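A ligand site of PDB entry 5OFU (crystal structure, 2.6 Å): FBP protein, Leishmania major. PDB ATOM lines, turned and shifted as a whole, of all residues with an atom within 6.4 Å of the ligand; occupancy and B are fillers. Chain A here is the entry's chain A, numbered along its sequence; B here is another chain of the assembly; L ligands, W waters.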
ATOM      1  N   GLU A  97      33.291 -33.857   2.324  1.00  0.00           N
ATOM      2  CA  GLU A  97      32.528 -33.581   1.091  1.00  0.00           C
ATOM      3  C   GLU A  97      33.357 -32.882   0.022  1.00  0.00           C
ATOM      4  O   GLU A  97      33.220 -33.194  -1.158  1.00  0.00           O
ATOM      5  CB  GLU A  97      31.282 -32.749   1.400  1.00  0.00           C
ATOM      6  CG  GLU A  97      30.554 -32.292   0.154  1.00  0.00           C
ATOM      7  CD  GLU A  97      29.084 -32.006   0.372  1.00  0.00           C
ATOM      8  OE1 GLU A  97      28.703 -31.587   1.480  1.00  0.00           O
ATOM      9  OE2 GLU A  97      28.316 -32.190  -0.588  1.00  0.00           O
ATOM     10  N   ASP A 118      30.633 -32.621   6.168  1.00  0.00           N
ATOM     11  CA  ASP A 118      30.820 -31.383   5.435  1.00  0.00           C
ATOM     12  C   ASP A 118      31.266 -30.373   6.496  1.00  0.00           C
ATOM     13  O   ASP A 118      30.460 -30.005   7.350  1.00  0.00           O
ATOM     14  CB  ASP A 118      29.511 -30.964   4.774  1.00  0.00           C
ATOM     15  CG  ASP A 118      29.656 -29.705   3.927  1.00  0.00           C
ATOM     16  OD1 ASP A 118      30.742 -29.095   3.940  1.00  0.00           O
ATOM     17  OD2 ASP A 118      28.650 -29.325   3.266  1.00  0.00           O
ATOM     18  N   LEU A 120      32.214 -27.150   6.395  1.00  0.00           N
ATOM     19  CA  LEU A 120      31.694 -25.787   6.268  1.00  0.00           C
ATOM     20  C   LEU A 120      30.600 -25.738   5.197  1.00  0.00           C
ATOM     21  O   LEU A 120      30.824 -25.394   4.042  1.00  0.00           O
ATOM     22  CB  LEU A 120      32.824 -24.793   5.990  1.00  0.00           C
ATOM     23  CG  LEU A 120      32.483 -23.308   6.191  1.00  0.00           C
ATOM     24  CD1 LEU A 120      31.993 -23.023   7.599  1.00  0.00           C
ATOM     25  CD2 LEU A 120      33.701 -22.445   5.873  1.00  0.00           C
ATOM     26  N   ASP A 121      29.411 -26.098   5.640  1.00  0.00           N
ATOM     27  CA  ASP A 121      28.197 -26.029   4.854  1.00  0.00           C
ATOM     28  C   ASP A 121      27.711 -24.595   4.706  1.00  0.00           C
ATOM     29  O   ASP A 121      27.800 -23.808   5.642  1.00  0.00           O
ATOM     30  CB  ASP A 121      27.116 -26.889   5.538  1.00  0.00           C
ATOM     31  CG  ASP A 121      25.772 -26.769   4.885  1.00  0.00           C
ATOM     32  OD1 ASP A 121      25.527 -27.446   3.859  1.00  0.00           O
ATOM     33  OD2 ASP A 121      24.923 -26.013   5.428  1.00  0.00           O
ATOM     34  N   GLY A 122      27.178 -24.284   3.526  1.00  0.00           N
ATOM     35  CA  GLY A 122      26.677 -22.940   3.212  1.00  0.00           C
ATOM     36  C   GLY A 122      27.797 -22.024   2.774  1.00  0.00           C
ATOM     37  O   GLY A 122      27.835 -20.865   3.164  1.00  0.00           O
ATOM     38  N   SER A 123      28.721 -22.553   1.965  1.00  0.00           N
ATOM     39  CA  SER A 123      29.936 -21.835   1.568  1.00  0.00           C
ATOM     40  C   SER A 123      29.689 -20.530   0.803  1.00  0.00           C
ATOM     41  O   SER A 123      30.520 -19.636   0.834  1.00  0.00           O
ATOM     42  CB  SER A 123      30.864 -22.739   0.750  1.00  0.00           C
ATOM     43  OG  SER A 123      30.294 -23.054  -0.506  1.00  0.00           O
ATOM     44  N   SER A 124      28.540 -20.427   0.129  1.00  0.00           N
ATOM     45  CA  SER A 124      28.143 -19.193  -0.545  1.00  0.00           C
ATOM     46  C   SER A 124      27.743 -18.075   0.440  1.00  0.00           C
ATOM     47  O   SER A 124      27.671 -16.907   0.022  1.00  0.00           O
ATOM     48  CB  SER A 124      27.014 -19.454  -1.544  1.00  0.00           C
ATOM     49  OG  SER A 124      25.739 -19.416  -0.903  1.00  0.00           O
ATOM     50  N   ILE A 135      28.356 -30.520   9.362  1.00  0.00           N
ATOM     51  CA  ILE A 135      27.463 -31.687   9.457  1.00  0.00           C
ATOM     52  C   ILE A 135      28.334 -32.932   9.467  1.00  0.00           C
ATOM     53  O   ILE A 135      29.308 -32.999   8.722  1.00  0.00           O
ATOM     54  CB  ILE A 135      26.514 -31.816   8.252  1.00  0.00           C
ATOM     55  CG1 ILE A 135      25.819 -30.519   7.929  1.00  0.00           C
ATOM     56  CG2 ILE A 135      25.432 -32.851   8.516  1.00  0.00           C
ATOM     57  CD1 ILE A 135      25.472 -30.414   6.455  1.00  0.00           C
ATOM     58  N   ASN A 218      14.796 -22.811  -2.780  1.00  0.00           N
ATOM     59  CA  ASN A 218      15.289 -21.773  -3.706  1.00  0.00           C
ATOM     60  C   ASN A 218      14.350 -21.634  -4.910  1.00  0.00           C
ATOM     61  O   ASN A 218      14.489 -22.367  -5.889  1.00  0.00           O
ATOM     62  CB  ASN A 218      16.722 -22.074  -4.174  1.00  0.00           C
ATOM     63  CG  ASN A 218      17.324 -20.945  -4.997  1.00  0.00           C
ATOM     64  OD1 ASN A 218      16.634 -20.021  -5.449  1.00  0.00           O
ATOM     65  ND2 ASN A 218      18.623 -21.000  -5.197  1.00  0.00           N
ATOM     66  N   ASN A 221      14.968 -21.417  -8.936  1.00  0.00           N
ATOM     67  CA  ASN A 221      14.932 -22.595  -9.820  1.00  0.00           C
ATOM     68  C   ASN A 221      13.513 -23.062 -10.206  1.00  0.00           C
ATOM     69  O   ASN A 221      13.357 -24.181 -10.691  1.00  0.00           O
ATOM     70  CB  ASN A 221      15.684 -23.763  -9.140  1.00  0.00           C
ATOM     71  CG  ASN A 221      17.139 -23.456  -8.863  1.00  0.00           C
ATOM     72  OD1 ASN A 221      17.617 -23.768  -7.791  1.00  0.00           O
ATOM     73  ND2 ASN A 221      17.847 -22.835  -9.808  1.00  0.00           N
ATOM     74  N   TYR A 248      14.680 -18.744   3.318  1.00  0.00           N
ATOM     75  CA  TYR A 248      15.787 -19.520   2.752  1.00  0.00           C
ATOM     76  C   TYR A 248      17.103 -18.764   2.930  1.00  0.00           C
ATOM     77  O   TYR A 248      17.416 -17.851   2.194  1.00  0.00           O
ATOM     78  CB  TYR A 248      15.512 -19.827   1.293  1.00  0.00           C
ATOM     79  CG  TYR A 248      16.422 -20.850   0.664  1.00  0.00           C
ATOM     80  CD1 TYR A 248      16.264 -22.214   0.925  1.00  0.00           C
ATOM     81  CD2 TYR A 248      17.408 -20.469  -0.238  1.00  0.00           C
ATOM     82  CE1 TYR A 248      17.073 -23.162   0.302  1.00  0.00           C
ATOM     83  CE2 TYR A 248      18.222 -21.404  -0.858  1.00  0.00           C
ATOM     84  CZ  TYR A 248      18.054 -22.744  -0.583  1.00  0.00           C
ATOM     85  OH  TYR A 248      18.844 -23.655  -1.219  1.00  0.00           O
ATOM     86  N   GLY A 250      20.086 -20.118   2.676  1.00  0.00           N
ATOM     87  CA  GLY A 250      21.106 -20.592   1.719  1.00  0.00           C
ATOM     88  C   GLY A 250      22.171 -21.517   2.320  1.00  0.00           C
ATOM     89  O   GLY A 250      23.113 -21.910   1.623  1.00  0.00           O
ATOM     90  N   SER A 251      22.052 -21.811   3.614  1.00  0.00           N
ATOM     91  CA  SER A 251      22.863 -22.818   4.281  1.00  0.00           C
ATOM     92  C   SER A 251      21.905 -23.852   4.820  1.00  0.00           C
ATOM     93  O   SER A 251      21.034 -23.529   5.626  1.00  0.00           O
ATOM     94  CB  SER A 251      23.677 -22.209   5.414  1.00  0.00           C
ATOM     95  OG  SER A 251      24.408 -21.081   4.950  1.00  0.00           O
ATOM     96  N   MET A 252      22.078 -25.098   4.381  1.00  0.00           N
ATOM     97  CA  MET A 252      21.222 -26.195   4.790  1.00  0.00           C
ATOM     98  C   MET A 252      21.159 -26.337   6.328  1.00  0.00           C
ATOM     99  O   MET A 252      20.089 -26.562   6.874  1.00  0.00           O
ATOM    100  CB  MET A 252      21.726 -27.505   4.174  1.00  0.00           C
ATOM    101  CG  MET A 252      20.781 -28.669   4.422  1.00  0.00           C
ATOM    102  SD  MET A 252      21.563 -30.272   4.255  1.00  0.00           S
ATOM    103  CE  MET A 252      20.112 -31.352   4.327  1.00  0.00           C
ATOM    104  N   VAL A 253      22.295 -26.155   7.002  1.00  0.00           N
ATOM    105  CA  VAL A 253      22.352 -26.268   8.455  1.00  0.00           C
ATOM    106  C   VAL A 253      21.538 -25.170   9.117  1.00  0.00           C
ATOM    107  O   VAL A 253      20.803 -25.447  10.050  1.00  0.00           O
ATOM    108  CB  VAL A 253      23.800 -26.293   8.977  1.00  0.00           C
ATOM    109  CG1 VAL A 253      23.825 -26.334  10.500  1.00  0.00           C
ATOM    110  CG2 VAL A 253      24.534 -27.515   8.449  1.00  0.00           C
ATOM    111  N   ASP A 255      18.942 -23.445   7.677  1.00  0.00           N
ATOM    112  CA  ASP A 255      17.533 -23.650   7.339  1.00  0.00           C
ATOM    113  C   ASP A 255      16.916 -24.821   8.107  1.00  0.00           C
ATOM    114  O   ASP A 255      15.805 -24.718   8.631  1.00  0.00           O
ATOM    115  CB  ASP A 255      17.350 -23.838   5.823  1.00  0.00           C
ATOM    116  CG  ASP A 255      17.626 -22.557   5.029  1.00  0.00           C
ATOM    117  OD1 ASP A 255      17.043 -21.495   5.380  1.00  0.00           O
ATOM    118  OD2 ASP A 255      18.408 -22.594   4.032  1.00  0.00           O
ATOM    119  N   PHE A 266      11.778 -28.002   4.563  1.00  0.00           N
ATOM    120  CA  PHE A 266      12.943 -27.641   3.760  1.00  0.00           C
ATOM    121  C   PHE A 266      12.979 -28.544   2.534  1.00  0.00           C
ATOM    122  O   PHE A 266      12.876 -29.767   2.661  1.00  0.00           O
ATOM    123  CB  PHE A 266      14.233 -27.803   4.588  1.00  0.00           C
ATOM    124  CG  PHE A 266      15.476 -27.508   3.812  1.00  0.00           C
ATOM    125  CD1 PHE A 266      15.902 -26.186   3.647  1.00  0.00           C
ATOM    126  CD2 PHE A 266      16.194 -28.529   3.193  1.00  0.00           C
ATOM    127  CE1 PHE A 266      17.025 -25.894   2.902  1.00  0.00           C
ATOM    128  CE2 PHE A 266      17.318 -28.247   2.452  1.00  0.00           C
ATOM    129  CZ  PHE A 266      17.744 -26.929   2.303  1.00  0.00           C
ATOM    130  N   TYR A 268      14.975 -29.318  -1.285  1.00  0.00           N
ATOM    131  CA  TYR A 268      15.838 -29.126  -2.421  1.00  0.00           C
ATOM    132  C   TYR A 268      15.489 -30.234  -3.429  1.00  0.00           C
ATOM    133  O   TYR A 268      16.055 -31.318  -3.371  1.00  0.00           O
ATOM    134  CB  TYR A 268      17.314 -29.127  -2.025  1.00  0.00           C
ATOM    135  CG  TYR A 268      18.131 -28.340  -3.020  1.00  0.00           C
ATOM    136  CD1 TYR A 268      18.182 -28.716  -4.355  1.00  0.00           C
ATOM    137  CD2 TYR A 268      18.825 -27.183  -2.637  1.00  0.00           C
ATOM    138  CE1 TYR A 268      18.892 -27.995  -5.289  1.00  0.00           C
ATOM    139  CE2 TYR A 268      19.540 -26.449  -3.567  1.00  0.00           C
ATOM    140  CZ  TYR A 268      19.568 -26.866  -4.890  1.00  0.00           C
ATOM    141  OH  TYR A 268      20.270 -26.198  -5.851  1.00  0.00           O
ATOM    142  N   GLN A 274      19.866 -30.563 -12.364  1.00  0.00           N
ATOM    143  CA  GLN A 274      20.234 -31.383 -11.218  1.00  0.00           C
ATOM    144  C   GLN A 274      19.198 -32.490 -11.084  1.00  0.00           C
ATOM    145  O   GLN A 274      18.297 -32.449 -10.252  1.00  0.00           O
ATOM    146  CB  GLN A 274      20.315 -30.509  -9.961  1.00  0.00           C
ATOM    147  CG  GLN A 274      21.256 -29.323 -10.111  1.00  0.00           C
ATOM    148  CD  GLN A 274      21.481 -28.579  -8.817  1.00  0.00           C
ATOM    149  OE1 GLN A 274      22.500 -28.784  -8.146  1.00  0.00           O
ATOM    150  NE2 GLN A 274      20.544 -27.720  -8.440  1.00  0.00           N
ATOM    151  N   LYS A 278      20.624 -31.661  -5.502  1.00  0.00           N
ATOM    152  CA  LYS A 278      21.973 -31.132  -5.224  1.00  0.00           C
ATOM    153  C   LYS A 278      22.694 -31.815  -4.044  1.00  0.00           C
ATOM    154  O   LYS A 278      23.905 -32.037  -4.111  1.00  0.00           O
ATOM    155  CB  LYS A 278      21.914 -29.628  -4.969  1.00  0.00           C
ATOM    156  CG  LYS A 278      23.288 -28.981  -4.915  1.00  0.00           C
ATOM    157  CD  LYS A 278      23.226 -27.539  -4.438  1.00  0.00           C
ATOM    158  CE  LYS A 278      24.629 -26.958  -4.338  1.00  0.00           C
ATOM    159  NZ  LYS A 278      24.635 -25.619  -3.718  1.00  0.00           N
ATOM    160  N   LEU A 279      21.986 -32.100  -2.957  1.00  0.00           N
ATOM    161  CA  LEU A 279      22.631 -32.408  -1.683  1.00  0.00           C
ATOM    162  C   LEU A 279      23.167 -33.823  -1.679  1.00  0.00           C
ATOM    163  O   LEU A 279      22.495 -34.742  -2.148  1.00  0.00           O
ATOM    164  CB  LEU A 279      21.669 -32.197  -0.515  1.00  0.00           C
ATOM    165  CG  LEU A 279      20.908 -30.865  -0.496  1.00  0.00           C
ATOM    166  CD1 LEU A 279      20.086 -30.761   0.775  1.00  0.00           C
ATOM    167  CD2 LEU A 279      21.832 -29.663  -0.623  1.00  0.00           C
ATOM    168  N   GLU A 284      25.531 -35.023   3.835  1.00  0.00           N
ATOM    169  CA  GLU A 284      24.547 -34.004   4.231  1.00  0.00           C
ATOM    170  C   GLU A 284      23.166 -34.577   4.517  1.00  0.00           C
ATOM    171  O   GLU A 284      22.658 -34.466   5.639  1.00  0.00           O
ATOM    172  CB  GLU A 284      24.432 -32.930   3.148  1.00  0.00           C
ATOM    173  CG  GLU A 284      25.744 -32.250   2.792  1.00  0.00           C
ATOM    174  CD  GLU A 284      25.574 -31.085   1.809  1.00  0.00           C
ATOM    175  OE1 GLU A 284      25.117 -31.342   0.653  1.00  0.00           O
ATOM    176  OE2 GLU A 284      25.906 -29.941   2.184  1.00  0.00           O
ATOM    177  N   SER B 245      19.157 -16.566  -8.430  1.00  0.00           N
ATOM    178  CA  SER B 245      19.140 -17.337  -7.195  1.00  0.00           C
ATOM    179  C   SER B 245      18.311 -16.571  -6.161  1.00  0.00           C
ATOM    180  O   SER B 245      18.367 -15.337  -6.115  1.00  0.00           O
ATOM    181  CB  SER B 245      20.566 -17.526  -6.708  1.00  0.00           C
ATOM    182  OG  SER B 245      20.610 -18.484  -5.668  1.00  0.00           O
ATOM    183  N   ALA B 246      17.552 -17.280  -5.331  1.00  0.00           N
ATOM    184  CA  ALA B 246      16.755 -16.657  -4.262  1.00  0.00           C
ATOM    185  C   ALA B 246      17.410 -16.823  -2.886  1.00  0.00           C
ATOM    186  O   ALA B 246      17.942 -17.895  -2.564  1.00  0.00           O
ATOM    187  CB  ALA B 246      15.365 -17.237  -4.242  1.00  0.00           C
ATOM    188  N   ARG B 247      17.381 -15.749  -2.097  1.00  0.00           N
ATOM    189  CA  ARG B 247      17.853 -15.759  -0.701  1.00  0.00           C
ATOM    190  C   ARG B 247      16.977 -14.865   0.131  1.00  0.00           C
ATOM    191  O   ARG B 247      16.723 -13.730  -0.226  1.00  0.00           O
ATOM    192  CB  ARG B 247      19.291 -15.231  -0.611  1.00  0.00           C
ATOM    193  CG  ARG B 247      20.363 -16.123  -1.223  1.00  0.00           C
ATOM    194  CD  ARG B 247      20.487 -17.412  -0.433  1.00  0.00           C
ATOM    195  NE  ARG B 247      21.587 -18.253  -0.904  1.00  0.00           N
ATOM    196  CZ  ARG B 247      21.514 -19.175  -1.869  1.00  0.00           C
ATOM    197  NH1 ARG B 247      20.382 -19.390  -2.577  1.00  0.00           N
ATOM    198  NH2 ARG B 247      22.602 -19.889  -2.152  1.00  0.00           N
HETATM  199  O1  LIG L   1      26.173 -27.325  -1.239  1.00  0.00           O
HETATM  200  C1  LIG L   1      25.288 -27.452  -0.125  1.00  0.00           C
HETATM  201  C2  LIG L   1      24.643 -26.103   0.156  1.00  0.00           C
HETATM  202  O2  LIG L   1      25.678 -25.169   0.513  1.00  0.00           O
HETATM  203  C3  LIG L   1      23.579 -26.161   1.251  1.00  0.00           C
HETATM  204  O3  LIG L   1      24.047 -25.657   2.505  1.00  0.00           O
HETATM  205  C4  LIG L   1      22.431 -25.331   0.744  1.00  0.00           C
HETATM  206  O4  LIG L   1      21.150 -25.852   1.087  1.00  0.00           O
HETATM  207  C5  LIG L   1      22.610 -25.332  -0.753  1.00  0.00           C
HETATM  208  O5  LIG L   1      23.985 -25.648  -1.027  1.00  0.00           O
HETATM  209  C6  LIG L   1      22.285 -23.987  -1.372  1.00  0.00           C
HETATM  210  O6  LIG L   1      22.155 -24.215  -2.774  1.00  0.00           O
HETATM  211  P1  LIG L   1      21.550 -23.103  -3.762  1.00  0.00           P
HETATM  212  O7  LIG L   1      22.644 -22.068  -3.876  1.00  0.00           O
HETATM  213  O8  LIG L   1      20.293 -22.631  -3.072  1.00  0.00           O
HETATM  214  O9  LIG L   1      21.368 -23.906  -5.027  1.00  0.00           O
HETATM  215  O   HOH W   1      23.497 -24.660  -6.000  1.00  0.00           O
HETATM  216  O   HOH W   2      19.922 -23.849   2.080  1.00  0.00           O
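The side-chain hydroxyl of Tyr 248 lies within hydrogen-bond range of an oxygen (O8) of the ligand (2.6 Å). The side-chain hydroxyl (OH) of Tyr 268 is in hydrogen-bond range of an oxygen (O9) of the ligand (2.7 Å). An oxygen (O3) of the ligand sits at hydrogen-bond distance from the side-chain carboxylate (OD1) of Asp 121 (2.7 Å). An oxygen (O9) of the ligand is in salt-bridge range of the side-chain amino group (NZ) of Lys 278, 3.9 Å away. An oxygen (O3) of the ligand sits at hydrogen-bond distance from the backbone NH of Met 252. The guanidinium group (NH2) of Arg 247 of chain B is in salt-bridge range of an oxygen (O7) of the ligand, 2.8 Å away. The side-chain amide nitrogen (ND2) of Asn 218 is in hydrogen-bond range of an oxygen (O8) of the ligand (3.2 Å). N of Gly 122 is in hydrogen-bond range of O2 of the ligand (3.5 Å).
The side-chain hydroxyl of Tyr 268 sits at hydrogen-bond distance from the side-chain amide nitrogen of Gln 274 (3.0 Å). The side-chain carboxylate (OD2) of Asp 121 is in hydrogen-bond range of the backbone NH (N) of Met 252 (3.2 Å). N of Val 253 is in hydrogen-bond range of OD2 of Asp 121 (3.1 Å). The guanidinium group of Arg 247 of chain B sits at hydrogen-bond distance from the side-chain hydroxyl of Ser 245 of chain B (3.2 Å). The guanidinium group (NH2) of Arg 247 of chain B lies within hydrogen-bond range of the side-chain hydroxyl (OG) of Ser 124. OG of Ser 245 of chain B is in hydrogen-bond range of ND2 of Asn 218, 3.2 Å away. The side-chain amide oxygen (OD1) of Asn 218 sits at hydrogen-bond distance from the backbone NH (N) of Ala 246 of chain B. OD2 of Asp 255 lies within hydrogen-bond range of N of Gly 250 (3.3 Å).
Residues that only touch the ligand: Glu 284, Ser 251, Gly 250 and Phe 266. Hydrophobic or aromatic side chains that line the ligand: Tyr 248, Met 252, Phe 266 and Tyr 268. Of the 25 residues printed, 12 come within 4 Å of the ligand. Along chain A the residues within 4 Å of the ligand span positions 121 to 284. The nearest printed residue that does not touch the ligand is Leu 279 (4.1 Å).
Water W1 lies within hydrogen-bond range of an oxygen (O9) of the ligand and the side-chain amino group of Lys 278. Water W2 lies within hydrogen-bond range of an oxygen (O4) of the ligand, the side-chain carboxylate (OD2) of Asp 255, the backbone NH (N) of Ser 251, the backbone NH (N) of Met 252 and the side-chain hydroxyl (OH) of Tyr 248.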
